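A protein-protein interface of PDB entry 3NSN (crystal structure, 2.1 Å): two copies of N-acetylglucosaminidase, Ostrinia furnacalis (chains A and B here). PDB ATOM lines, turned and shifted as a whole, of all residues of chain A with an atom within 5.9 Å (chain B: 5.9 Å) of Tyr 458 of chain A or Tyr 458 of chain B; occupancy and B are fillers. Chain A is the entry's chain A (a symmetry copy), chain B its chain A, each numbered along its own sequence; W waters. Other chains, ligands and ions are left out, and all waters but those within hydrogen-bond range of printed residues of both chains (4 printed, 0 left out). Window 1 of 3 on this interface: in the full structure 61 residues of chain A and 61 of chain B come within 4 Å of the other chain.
The side-chain amide nitrogen (ND2) of Asn 466 of chain B sits at hydrogen-bond distance from the backbone carbonyl oxygen (O) of Tyr 472 of chain A, 3.1 Å away. The side-chain amide nitrogen (ND2) of Asn 466 of chain A is in hydrogen-bond range of the backbone carbonyl oxygen (O) of Tyr 472 of chain B. OE1 of Glu 556 of chain A lies within salt-bridge range of NH1 of Arg 514 of chain B, at 2.9 Å. OE1 of Glu 556 of chain B lies within salt-bridge range of NH1 of Arg 514 of chain A, at 2.9 Å.
NH1 of Arg 514 of chain A sits at hydrogen-bond distance from OH of Tyr 458 of chain A, at 3.2 Å. The side-chain amide nitrogen (ND2) of Asn 466 of chain B sits at hydrogen-bond distance from the backbone carbonyl oxygen (O) of Tyr 458 of chain B (3.1 Å). The backbone NH (N) of Asn 467 of chain A lies within hydrogen-bond range of the backbone carbonyl oxygen (O) of Tyr 458 of chain A (2.9 Å). The guanidinium group (NE) of Arg 518 of chain B sits close to the side-chain hydroxyl (OH) of Tyr 472 of chain B (3.2 Å). NH2 of Arg 514 of chain A sits at hydrogen-bond distance from O of Gln 505 of chain A, 3.0 Å away. NH2 of Arg 518 of chain A is in hydrogen-bond range of O of Arg 514 of chain A (3.0 Å).
Among the printed residues, merely in contact across the chains: Gly 457 of chain A with Tyr 472 of chain B (3.3 Å), Tyr 458 of chain A with Tyr 458 of chain B (3.98 Å), Tyr 458 of chain A with Tyr 472 of chain B (3.8 Å), Gly 459 of chain A with Tyr 472 of chain B (3.6 Å), Tyr 472 of chain A with Gly 457 of chain B (3.3 Å), Tyr 472 of chain A with Tyr 458 of chain B (3.8 Å) and Tyr 472 of chain A with Gly 459 of chain B (3.6 Å).
Printed residues of chain B within 4 Å of Gly 457 of chain A: Tyr 472. Of chain B, only Tyr 458 (3.98 Å) and Tyr 472 (3.8 Å) come within 4 Å of Tyr 458 of chain A. Of chain A, only Tyr 458 (3.98 Å) and Tyr 472 (3.8 Å) come within 4 Å of Tyr 458 of chain B. Gly 465 of chain B touches none of the printed residues of chain A. Of the printed residues of chain A, Asn 466 of chain B touches Tyr 472. The nearest residue of chain B that does not touch Tyr 458 of chain A is Glu 556 of chain B (4.3 Å).
Hydrophobic or aromatic side chains of chain B within 4 Å of the printed part of chain A: Tyr 458 and Tyr 472. Among the printed residues, 11 pairs touch across the chains.
Tyr 458 of chain A touches Tyr 472 of chain B, and with the chains exchanged Tyr 472 of chain A touches Tyr 458 of chain B. Gly 459 of chain A touches Tyr 472 of chain B, and with the chains exchanged Tyr 472 of chain A touches Gly 459 of chain B. Asn 466 of chain A touches Tyr 472 of chain B, and with the chains exchanged Tyr 472 of chain A touches Asn 466 of chain B. Arg 514 of chain A touches Glu 556 of chain B, and with the chains exchanged Glu 556 of chain A touches Arg 514 of chain B. 16 positions are printed for both chains.
Water W4 bridges OD1 of Asn 466 of chain A (2.6 Å) and O of Tyr 472 of chain B (3.0 Å). Water W2 lies within hydrogen-bond range of the side-chain amide oxygen of Asn 466 of chain B (2.6 Å) and the backbone carbonyl oxygen of Tyr 472 of chain A (3.0 Å). Water W3 bridges the backbone carbonyl oxygen (O) of Gly 457 of chain A and the backbone NH (N) of Tyr 472 of chain B. Water W1 bridges the backbone carbonyl oxygen (O) of Gly 457 of chain B and the backbone NH (N) of Tyr 472 of chain A.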
ATOM      1  N   PHE A 454      27.035  -7.687 -16.273  1.00  0.00           N
ATOM      2  CA  PHE A 454      26.544  -8.110 -14.977  1.00  0.00           C
ATOM      3  C   PHE A 454      25.031  -8.215 -14.819  1.00  0.00           C
ATOM      4  O   PHE A 454      24.560  -8.877 -13.961  1.00  0.00           O
ATOM      5  CB  PHE A 454      27.222  -7.352 -13.860  1.00  0.00           C
ATOM      6  CG  PHE A 454      28.601  -7.846 -13.521  1.00  0.00           C
ATOM      7  CD1 PHE A 454      29.336  -8.618 -14.394  1.00  0.00           C
ATOM      8  CD2 PHE A 454      29.192  -7.475 -12.372  1.00  0.00           C
ATOM      9  CE1 PHE A 454      30.584  -9.025 -14.066  1.00  0.00           C
ATOM     10  CE2 PHE A 454      30.424  -7.891 -12.073  1.00  0.00           C
ATOM     11  CZ  PHE A 454      31.113  -8.641 -12.906  1.00  0.00           C
ATOM     12  N   ASP A 455      24.309  -7.536 -15.695  1.00  0.00           N
ATOM     13  CA  ASP A 455      22.882  -7.569 -15.805  1.00  0.00           C
ATOM     14  C   ASP A 455      22.232  -8.818 -16.365  1.00  0.00           C
ATOM     15  O   ASP A 455      21.117  -9.099 -16.055  1.00  0.00           O
ATOM     16  CB  ASP A 455      22.365  -6.338 -16.498  1.00  0.00           C
ATOM     17  CG  ASP A 455      22.880  -6.195 -17.873  1.00  0.00           C
ATOM     18  OD1 ASP A 455      24.054  -6.408 -18.106  1.00  0.00           O
ATOM     19  OD2 ASP A 455      22.108  -5.853 -18.703  1.00  0.00           O
ATOM     20  N   CYS A 456      22.962  -9.573 -17.175  1.00  0.00           N
ATOM     21  CA  CYS A 456      22.427 -10.713 -17.897  1.00  0.00           C
ATOM     22  C   CYS A 456      21.906 -11.830 -17.022  1.00  0.00           C
ATOM     23  O   CYS A 456      22.371 -12.025 -15.960  1.00  0.00           O
ATOM     24  CB  CYS A 456      23.485 -11.320 -18.824  1.00  0.00           C
ATOM     25  SG  CYS A 456      24.450 -10.263 -19.964  1.00  0.00           S
ATOM     26  N   GLY A 457      20.944 -12.564 -17.537  1.00  0.00           N
ATOM     27  CA  GLY A 457      20.406 -13.777 -16.956  1.00  0.00           C
ATOM     28  C   GLY A 457      19.099 -13.862 -16.207  1.00  0.00           C
ATOM     29  O   GLY A 457      18.543 -14.895 -16.041  1.00  0.00           O
ATOM     30  N   TYR A 458      18.571 -12.736 -15.835  1.00  0.00           N
ATOM     31  CA  TYR A 458      17.337 -12.664 -15.128  1.00  0.00           C
ATOM     32  C   TYR A 458      16.137 -12.771 -16.050  1.00  0.00           C
ATOM     33  O   TYR A 458      16.284 -12.967 -17.202  1.00  0.00           O
ATOM     34  CB  TYR A 458      17.312 -11.359 -14.388  1.00  0.00           C
ATOM     35  CG  TYR A 458      18.338 -11.364 -13.363  1.00  0.00           C
ATOM     36  CD1 TYR A 458      18.087 -11.922 -12.176  1.00  0.00           C
ATOM     37  CD2 TYR A 458      19.586 -10.897 -13.618  1.00  0.00           C
ATOM     38  CE1 TYR A 458      18.993 -11.971 -11.264  1.00  0.00           C
ATOM     39  CE2 TYR A 458      20.485 -10.964 -12.733  1.00  0.00           C
ATOM     40  CZ  TYR A 458      20.184 -11.512 -11.564  1.00  0.00           C
ATOM     41  OH  TYR A 458      21.082 -11.562 -10.659  1.00  0.00           O
ATOM     42  N   GLY A 459      14.961 -12.583 -15.515  1.00  0.00           N
ATOM     43  CA  GLY A 459      13.750 -12.615 -16.302  1.00  0.00           C
ATOM     44  C   GLY A 459      13.635 -11.482 -17.309  1.00  0.00           C
ATOM     45  O   GLY A 459      14.291 -10.529 -17.181  1.00  0.00           O
ATOM     46  N   ALA A 460      12.806 -11.640 -18.314  1.00  0.00           N
ATOM     47  CA  ALA A 460      12.586 -10.588 -19.294  1.00  0.00           C
ATOM     48  C   ALA A 460      11.921  -9.387 -18.635  1.00  0.00           C
ATOM     49  O   ALA A 460      11.207  -9.560 -17.736  1.00  0.00           O
ATOM     50  CB  ALA A 460      11.725 -11.093 -20.431  1.00  0.00           C
ATOM     51  N   GLY A 465      10.032 -14.794 -20.583  1.00  0.00           N
ATOM     52  CA  GLY A 465      11.280 -15.450 -20.822  1.00  0.00           C
ATOM     53  C   GLY A 465      12.387 -14.857 -19.978  1.00  0.00           C
ATOM     54  O   GLY A 465      12.223 -14.634 -18.816  1.00  0.00           O
ATOM     55  N   ASN A 466      13.517 -14.600 -20.591  1.00  0.00           N
ATOM     56  CA  ASN A 466      14.697 -14.140 -19.901  1.00  0.00           C
ATOM     57  C   ASN A 466      15.254 -12.926 -20.593  1.00  0.00           C
ATOM     58  O   ASN A 466      14.884 -12.677 -21.686  1.00  0.00           O
ATOM     59  CB  ASN A 466      15.728 -15.271 -19.817  1.00  0.00           C
ATOM     60  CG  ASN A 466      15.397 -16.307 -18.746  1.00  0.00           C
ATOM     61  OD1 ASN A 466      14.960 -17.356 -19.041  1.00  0.00           O
ATOM     62  ND2 ASN A 466      15.612 -15.977 -17.528  1.00  0.00           N
ATOM     63  N   ASN A 467      16.131 -12.169 -19.954  1.00  0.00           N
ATOM     64  CA  ASN A 467      16.694 -10.955 -20.586  1.00  0.00           C
ATOM     65  C   ASN A 467      17.662 -11.193 -21.768  1.00  0.00           C
ATOM     66  O   ASN A 467      18.115 -12.284 -21.986  1.00  0.00           O
ATOM     67  CB  ASN A 467      17.217  -9.931 -19.589  1.00  0.00           C
ATOM     68  CG  ASN A 467      18.440 -10.384 -18.834  1.00  0.00           C
ATOM     69  OD1 ASN A 467      19.262 -11.101 -19.327  1.00  0.00           O
ATOM     70  ND2 ASN A 467      18.538  -9.951 -17.621  1.00  0.00           N
ATOM     71  N   SER A 470      21.110 -13.269 -21.633  1.00  0.00           N
ATOM     72  CA  SER A 470      21.126 -14.415 -20.784  1.00  0.00           C
ATOM     73  C   SER A 470      21.898 -15.512 -21.504  1.00  0.00           C
ATOM     74  O   SER A 470      21.970 -15.485 -22.711  1.00  0.00           O
ATOM     75  CB  SER A 470      19.718 -14.887 -20.483  1.00  0.00           C
ATOM     76  OG  SER A 470      19.043 -14.002 -19.663  1.00  0.00           O
ATOM     77  N   TYR A 472      23.083 -16.036 -17.100  1.00  0.00           N
ATOM     78  CA  TYR A 472      23.824 -15.376 -16.058  1.00  0.00           C
ATOM     79  C   TYR A 472      25.301 -15.716 -16.135  1.00  0.00           C
ATOM     80  O   TYR A 472      25.661 -16.834 -16.266  1.00  0.00           O
ATOM     81  CB  TYR A 472      23.241 -15.761 -14.683  1.00  0.00           C
ATOM     82  CG  TYR A 472      23.852 -15.108 -13.507  1.00  0.00           C
ATOM     83  CD1 TYR A 472      24.881 -15.678 -12.836  1.00  0.00           C
ATOM     84  CD2 TYR A 472      23.384 -13.915 -13.050  1.00  0.00           C
ATOM     85  CE1 TYR A 472      25.430 -15.082 -11.766  1.00  0.00           C
ATOM     86  CE2 TYR A 472      23.915 -13.322 -11.990  1.00  0.00           C
ATOM     87  CZ  TYR A 472      24.945 -13.896 -11.339  1.00  0.00           C
ATOM     88  OH  TYR A 472      25.504 -13.292 -10.275  1.00  0.00           O
ATOM     89  N   GLN A 505      16.970  -3.737 -14.823  1.00  0.00           N
ATOM     90  CA  GLN A 505      16.583  -4.629 -13.795  1.00  0.00           C
ATOM     91  C   GLN A 505      17.460  -4.570 -12.571  1.00  0.00           C
ATOM     92  O   GLN A 505      17.721  -5.568 -11.993  1.00  0.00           O
ATOM     93  CB  GLN A 505      16.548  -6.020 -14.341  1.00  0.00           C
ATOM     94  CG  GLN A 505      15.526  -6.183 -15.392  1.00  0.00           C
ATOM     95  CD  GLN A 505      15.553  -7.504 -16.007  1.00  0.00           C
ATOM     96  OE1 GLN A 505      16.329  -7.728 -16.833  1.00  0.00           O
ATOM     97  NE2 GLN A 505      14.717  -8.382 -15.592  1.00  0.00           N
ATOM     98  N   ARG A 514      24.536  -7.782  -7.572  1.00  0.00           N
ATOM     99  CA  ARG A 514      24.893  -7.703  -8.975  1.00  0.00           C
ATOM    100  C   ARG A 514      26.412  -7.571  -9.132  1.00  0.00           C
ATOM    101  O   ARG A 514      26.975  -8.220  -9.927  1.00  0.00           O
ATOM    102  CB  ARG A 514      24.189  -6.547  -9.710  1.00  0.00           C
ATOM    103  CG  ARG A 514      22.736  -6.673  -9.988  1.00  0.00           C
ATOM    104  CD  ARG A 514      22.429  -7.682 -11.010  1.00  0.00           C
ATOM    105  NE  ARG A 514      21.049  -7.755 -11.433  1.00  0.00           N
ATOM    106  CZ  ARG A 514      20.036  -8.248 -10.736  1.00  0.00           C
ATOM    107  NH1 ARG A 514      20.161  -8.739  -9.535  1.00  0.00           N
ATOM    108  NH2 ARG A 514      18.879  -8.267 -11.285  1.00  0.00           N
ATOM    109  N   ARG A 518      31.476 -10.877  -8.122  1.00  0.00           N
ATOM    110  CA  ARG A 518      31.905 -11.065  -9.472  1.00  0.00           C
ATOM    111  C   ARG A 518      32.913 -10.043  -9.941  1.00  0.00           C
ATOM    112  O   ARG A 518      33.828 -10.376 -10.617  1.00  0.00           O
ATOM    113  CB  ARG A 518      30.721 -11.162 -10.414  1.00  0.00           C
ATOM    114  CG  ARG A 518      30.037 -12.496 -10.445  1.00  0.00           C
ATOM    115  CD  ARG A 518      28.898 -12.548 -11.453  1.00  0.00           C
ATOM    116  NE  ARG A 518      27.915 -11.503 -11.321  1.00  0.00           N
ATOM    117  CZ  ARG A 518      26.960 -11.240 -12.191  1.00  0.00           C
ATOM    118  NH1 ARG A 518      26.801 -11.930 -13.260  1.00  0.00           N
ATOM    119  NH2 ARG A 518      26.164 -10.274 -11.964  1.00  0.00           N
ATOM    120  N   GLU A 556      26.627 -11.762  -3.302  1.00  0.00           N
ATOM    121  CA  GLU A 556      26.048 -12.982  -3.767  1.00  0.00           C
ATOM    122  C   GLU A 556      26.771 -14.097  -3.074  1.00  0.00           C
ATOM    123  O   GLU A 556      27.898 -13.971  -2.748  1.00  0.00           O
ATOM    124  CB  GLU A 556      26.288 -13.145  -5.239  1.00  0.00           C
ATOM    125  CG  GLU A 556      25.118 -12.839  -6.126  1.00  0.00           C
ATOM    126  CD  GLU A 556      23.879 -13.605  -5.745  1.00  0.00           C
ATOM    127  OE1 GLU A 556      22.820 -13.054  -5.698  1.00  0.00           O
ATOM    128  OE2 GLU A 556      23.991 -14.777  -5.497  1.00  0.00           O
ATOM    129  N   PHE B 454      13.419 -21.294  -6.807  1.00  0.00           N
ATOM    130  CA  PHE B 454      13.942 -19.945  -6.726  1.00  0.00           C
ATOM    131  C   PHE B 454      15.456 -19.792  -6.812  1.00  0.00           C
ATOM    132  O   PHE B 454      15.940 -18.758  -7.116  1.00  0.00           O
ATOM    133  CB  PHE B 454      13.315 -19.183  -5.583  1.00  0.00           C
ATOM    134  CG  PHE B 454      11.938 -18.653  -5.869  1.00  0.00           C
ATOM    135  CD1 PHE B 454      11.159 -19.154  -6.889  1.00  0.00           C
ATOM    136  CD2 PHE B 454      11.391 -17.716  -5.075  1.00  0.00           C
ATOM    137  CE1 PHE B 454       9.913 -18.671  -7.103  1.00  0.00           C
ATOM    138  CE2 PHE B 454      10.160 -17.256  -5.308  1.00  0.00           C
ATOM    139  CZ  PHE B 454       9.430 -17.731  -6.295  1.00  0.00           C
ATOM    140  N   ASP B 455      16.164 -20.874  -6.535  1.00  0.00           N
ATOM    141  CA  ASP B 455      17.586 -20.993  -6.651  1.00  0.00           C
ATOM    142  C   ASP B 455      18.191 -21.055  -8.040  1.00  0.00           C
ATOM    143  O   ASP B 455      19.309 -20.685  -8.218  1.00  0.00           O
ATOM    144  CB  ASP B 455      18.107 -22.110  -5.789  1.00  0.00           C
ATOM    145  CG  ASP B 455      17.552 -23.426  -6.158  1.00  0.00           C
ATOM    146  OD1 ASP B 455      16.367 -23.537  -6.406  1.00  0.00           O
ATOM    147  OD2 ASP B 455      18.305 -24.340  -6.179  1.00  0.00           O
ATOM    148  N   CYS B 456      17.420 -21.505  -9.021  1.00  0.00           N
ATOM    149  CA  CYS B 456      17.908 -21.755 -10.365  1.00  0.00           C
ATOM    150  C   CYS B 456      18.433 -20.535 -11.086  1.00  0.00           C
ATOM    151  O   CYS B 456      17.998 -19.468 -10.852  1.00  0.00           O
ATOM    152  CB  CYS B 456      16.809 -22.362 -11.243  1.00  0.00           C
ATOM    153  SG  CYS B 456      15.831 -23.796 -10.663  1.00  0.00           S
ATOM    154  N   GLY B 457      19.362 -20.755 -11.990  1.00  0.00           N
ATOM    155  CA  GLY B 457      19.892 -19.771 -12.911  1.00  0.00           C
ATOM    156  C   GLY B 457      21.221 -19.073 -12.750  1.00  0.00           C
ATOM    157  O   GLY B 457      21.759 -18.542 -13.662  1.00  0.00           O
ATOM    158  N   TYR B 458      21.783 -19.164 -11.584  1.00  0.00           N
ATOM    159  CA  TYR B 458      23.041 -18.563 -11.290  1.00  0.00           C
ATOM    160  C   TYR B 458      24.208 -19.402 -11.774  1.00  0.00           C
ATOM    161  O   TYR B 458      24.021 -20.392 -12.385  1.00  0.00           O
ATOM    162  CB  TYR B 458      23.116 -18.370  -9.804  1.00  0.00           C
ATOM    163  CG  TYR B 458      22.123 -17.397  -9.390  1.00  0.00           C
ATOM    164  CD1 TYR B 458      22.399 -16.093  -9.469  1.00  0.00           C
ATOM    165  CD2 TYR B 458      20.878 -17.783  -9.014  1.00  0.00           C
ATOM    166  CE1 TYR B 458      21.522 -15.212  -9.141  1.00  0.00           C
ATOM    167  CE2 TYR B 458      20.007 -16.920  -8.716  1.00  0.00           C
ATOM    168  CZ  TYR B 458      20.332 -15.637  -8.792  1.00  0.00           C
ATOM    169  OH  TYR B 458      19.462 -14.761  -8.469  1.00  0.00           O
ATOM    170  N   GLY B 459      25.404 -19.003 -11.435  1.00  0.00           N
ATOM    171  CA  GLY B 459      26.589 -19.745 -11.799  1.00  0.00           C
ATOM    172  C   GLY B 459      26.696 -21.107 -11.133  1.00  0.00           C
ATOM    173  O   GLY B 459      26.065 -21.334 -10.181  1.00  0.00           O
ATOM    174  N   ALA B 460      27.489 -21.995 -11.683  1.00  0.00           N
ATOM    175  CA  ALA B 460      27.701 -23.304 -11.085  1.00  0.00           C
ATOM    176  C   ALA B 460      28.412 -23.161  -9.746  1.00  0.00           C
ATOM    177  O   ALA B 460      29.150 -22.278  -9.590  1.00  0.00           O
ATOM    178  CB  ALA B 460      28.515 -24.185 -12.008  1.00  0.00           C
ATOM    179  N   GLY B 465      30.123 -22.966 -15.546  1.00  0.00           N
ATOM    180  CA  GLY B 465      28.855 -22.914 -16.204  1.00  0.00           C
ATOM    181  C   GLY B 465      27.787 -22.332 -15.301  1.00  0.00           C
ATOM    182  O   GLY B 465      27.992 -21.344 -14.663  1.00  0.00           O
ATOM    183  N   ASN B 466      26.644 -22.973 -15.259  1.00  0.00           N
ATOM    184  CA  ASN B 466      25.497 -22.482 -14.535  1.00  0.00           C
ATOM    185  C   ASN B 466      24.944 -23.569 -13.655  1.00  0.00           C
ATOM    186  O   ASN B 466      25.284 -24.683 -13.847  1.00  0.00           O
ATOM    187  CB  ASN B 466      24.445 -21.956 -15.519  1.00  0.00           C
ATOM    188  CG  ASN B 466      24.788 -20.581 -16.085  1.00  0.00           C
ATOM    189  OD1 ASN B 466      25.193 -20.468 -17.182  1.00  0.00           O
ATOM    190  ND2 ASN B 466      24.619 -19.573 -15.315  1.00  0.00           N
ATOM    191  N   ASN B 467      24.104 -23.244 -12.685  1.00  0.00           N
ATOM    192  CA  ASN B 467      23.547 -24.275 -11.782  1.00  0.00           C
ATOM    193  C   ASN B 467      22.537 -25.259 -12.416  1.00  0.00           C
ATOM    194  O   ASN B 467      22.055 -25.040 -13.494  1.00  0.00           O
ATOM    195  CB  ASN B 467      23.078 -23.727 -10.441  1.00  0.00           C
ATOM    196  CG  ASN B 467      21.870 -22.832 -10.538  1.00  0.00           C
ATOM    197  OD1 ASN B 467      21.018 -23.000 -11.362  1.00  0.00           O
ATOM    198  ND2 ASN B 467      21.820 -21.869  -9.678  1.00  0.00           N
ATOM    199  N   SER B 470      19.053 -24.278 -14.179  1.00  0.00           N
ATOM    200  CA  SER B 470      19.039 -23.059 -14.920  1.00  0.00           C
ATOM    201  C   SER B 470      18.222 -23.297 -16.182  1.00  0.00           C
ATOM    202  O   SER B 470      18.112 -24.423 -16.610  1.00  0.00           O
ATOM    203  CB  SER B 470      20.445 -22.633 -15.289  1.00  0.00           C
ATOM    204  OG  SER B 470      21.164 -22.222 -14.181  1.00  0.00           O
ATOM    205  N   TYR B 472      17.164 -18.996 -14.973  1.00  0.00           N
ATOM    206  CA  TYR B 472      16.471 -18.265 -13.947  1.00  0.00           C
ATOM    207  C   TYR B 472      14.986 -18.176 -14.244  1.00  0.00           C
ATOM    208  O   TYR B 472      14.598 -17.868 -15.317  1.00  0.00           O
ATOM    209  CB  TYR B 472      17.089 -16.858 -13.804  1.00  0.00           C
ATOM    210  CG  TYR B 472      16.529 -16.003 -12.738  1.00  0.00           C
ATOM    211  CD1 TYR B 472      15.510 -15.144 -12.980  1.00  0.00           C
ATOM    212  CD2 TYR B 472      17.037 -16.039 -11.476  1.00  0.00           C
ATOM    213  CE1 TYR B 472      15.008 -14.367 -12.009  1.00  0.00           C
ATOM    214  CE2 TYR B 472      16.552 -15.270 -10.511  1.00  0.00           C
ATOM    215  CZ  TYR B 472      15.531 -14.429 -10.765  1.00  0.00           C
ATOM    216  OH  TYR B 472      15.019 -13.660  -9.787  1.00  0.00           O
ATOM    217  N   GLN B 505      23.606 -21.655  -2.921  1.00  0.00           N
ATOM    218  CA  GLN B 505      24.006 -20.374  -3.372  1.00  0.00           C
ATOM    219  C   GLN B 505      23.169 -19.245  -2.829  1.00  0.00           C
ATOM    220  O   GLN B 505      22.906 -18.328  -3.528  1.00  0.00           O
ATOM    221  CB  GLN B 505      23.994 -20.356  -4.866  1.00  0.00           C
ATOM    222  CG  GLN B 505      24.980 -21.289  -5.445  1.00  0.00           C
ATOM    223  CD  GLN B 505      24.905 -21.360  -6.899  1.00  0.00           C
ATOM    224  OE1 GLN B 505      24.099 -22.025  -7.393  1.00  0.00           O
ATOM    225  NE2 GLN B 505      25.735 -20.663  -7.582  1.00  0.00           N
ATOM    226  N   ARG B 514      16.188 -13.255  -3.700  1.00  0.00           N
ATOM    227  CA  ARG B 514      15.788 -14.576  -4.143  1.00  0.00           C
ATOM    228  C   ARG B 514      14.269 -14.739  -4.032  1.00  0.00           C
ATOM    229  O   ARG B 514      13.667 -15.218  -4.914  1.00  0.00           O
ATOM    230  CB  ARG B 514      16.494 -15.707  -3.371  1.00  0.00           C
ATOM    231  CG  ARG B 514      17.934 -15.948  -3.638  1.00  0.00           C
ATOM    232  CD  ARG B 514      18.187 -16.521  -4.967  1.00  0.00           C
ATOM    233  NE  ARG B 514      19.552 -16.914  -5.236  1.00  0.00           N
ATOM    234  CZ  ARG B 514      20.576 -16.105  -5.463  1.00  0.00           C
ATOM    235  NH1 ARG B 514      20.478 -14.805  -5.461  1.00  0.00           N
ATOM    236  NH2 ARG B 514      21.714 -16.630  -5.724  1.00  0.00           N
ATOM    237  N   ARG B 518       9.171 -12.450  -6.553  1.00  0.00           N
ATOM    238  CA  ARG B 518       8.695 -13.620  -7.222  1.00  0.00           C
ATOM    239  C   ARG B 518       7.695 -14.418  -6.420  1.00  0.00           C
ATOM    240  O   ARG B 518       6.752 -14.899  -6.954  1.00  0.00           O
ATOM    241  CB  ARG B 518       9.847 -14.480  -7.704  1.00  0.00           C
ATOM    242  CG  ARG B 518      10.501 -14.021  -8.972  1.00  0.00           C
ATOM    243  CD  ARG B 518      11.606 -14.959  -9.435  1.00  0.00           C
ATOM    244  NE  ARG B 518      12.614 -15.252  -8.449  1.00  0.00           N
ATOM    245  CZ  ARG B 518      13.547 -16.176  -8.563  1.00  0.00           C
ATOM    246  NH1 ARG B 518      13.658 -16.910  -9.609  1.00  0.00           N
ATOM    247  NH2 ARG B 518      14.370 -16.348  -7.608  1.00  0.00           N
ATOM    248  N   GLU B 556      14.148  -7.756  -5.712  1.00  0.00           N
ATOM    249  CA  GLU B 556      14.687  -7.739  -7.034  1.00  0.00           C
ATOM    250  C   GLU B 556      13.963  -6.661  -7.783  1.00  0.00           C
ATOM    251  O   GLU B 556      12.850  -6.383  -7.509  1.00  0.00           O
ATOM    252  CB  GLU B 556      14.397  -9.036  -7.732  1.00  0.00           C
ATOM    253  CG  GLU B 556      15.545  -9.997  -7.819  1.00  0.00           C
ATOM    254  CD  GLU B 556      16.779  -9.382  -8.424  1.00  0.00           C
ATOM    255  OE1 GLU B 556      17.850  -9.568  -7.930  1.00  0.00           O
ATOM    256  OE2 GLU B 556      16.649  -8.707  -9.412  1.00  0.00           O
HETATM  257  O   HOH W   1      21.324 -18.446 -16.295  1.00  0.00           O
HETATM  258  O   HOH W   2      27.226 -18.932 -17.785  1.00  0.00           O
HETATM  259  O   HOH W   3      18.897 -17.379 -16.957  1.00  0.00           O
HETATM  260  O   HOH W   4      12.941 -18.450 -17.782  1.00  0.00           O
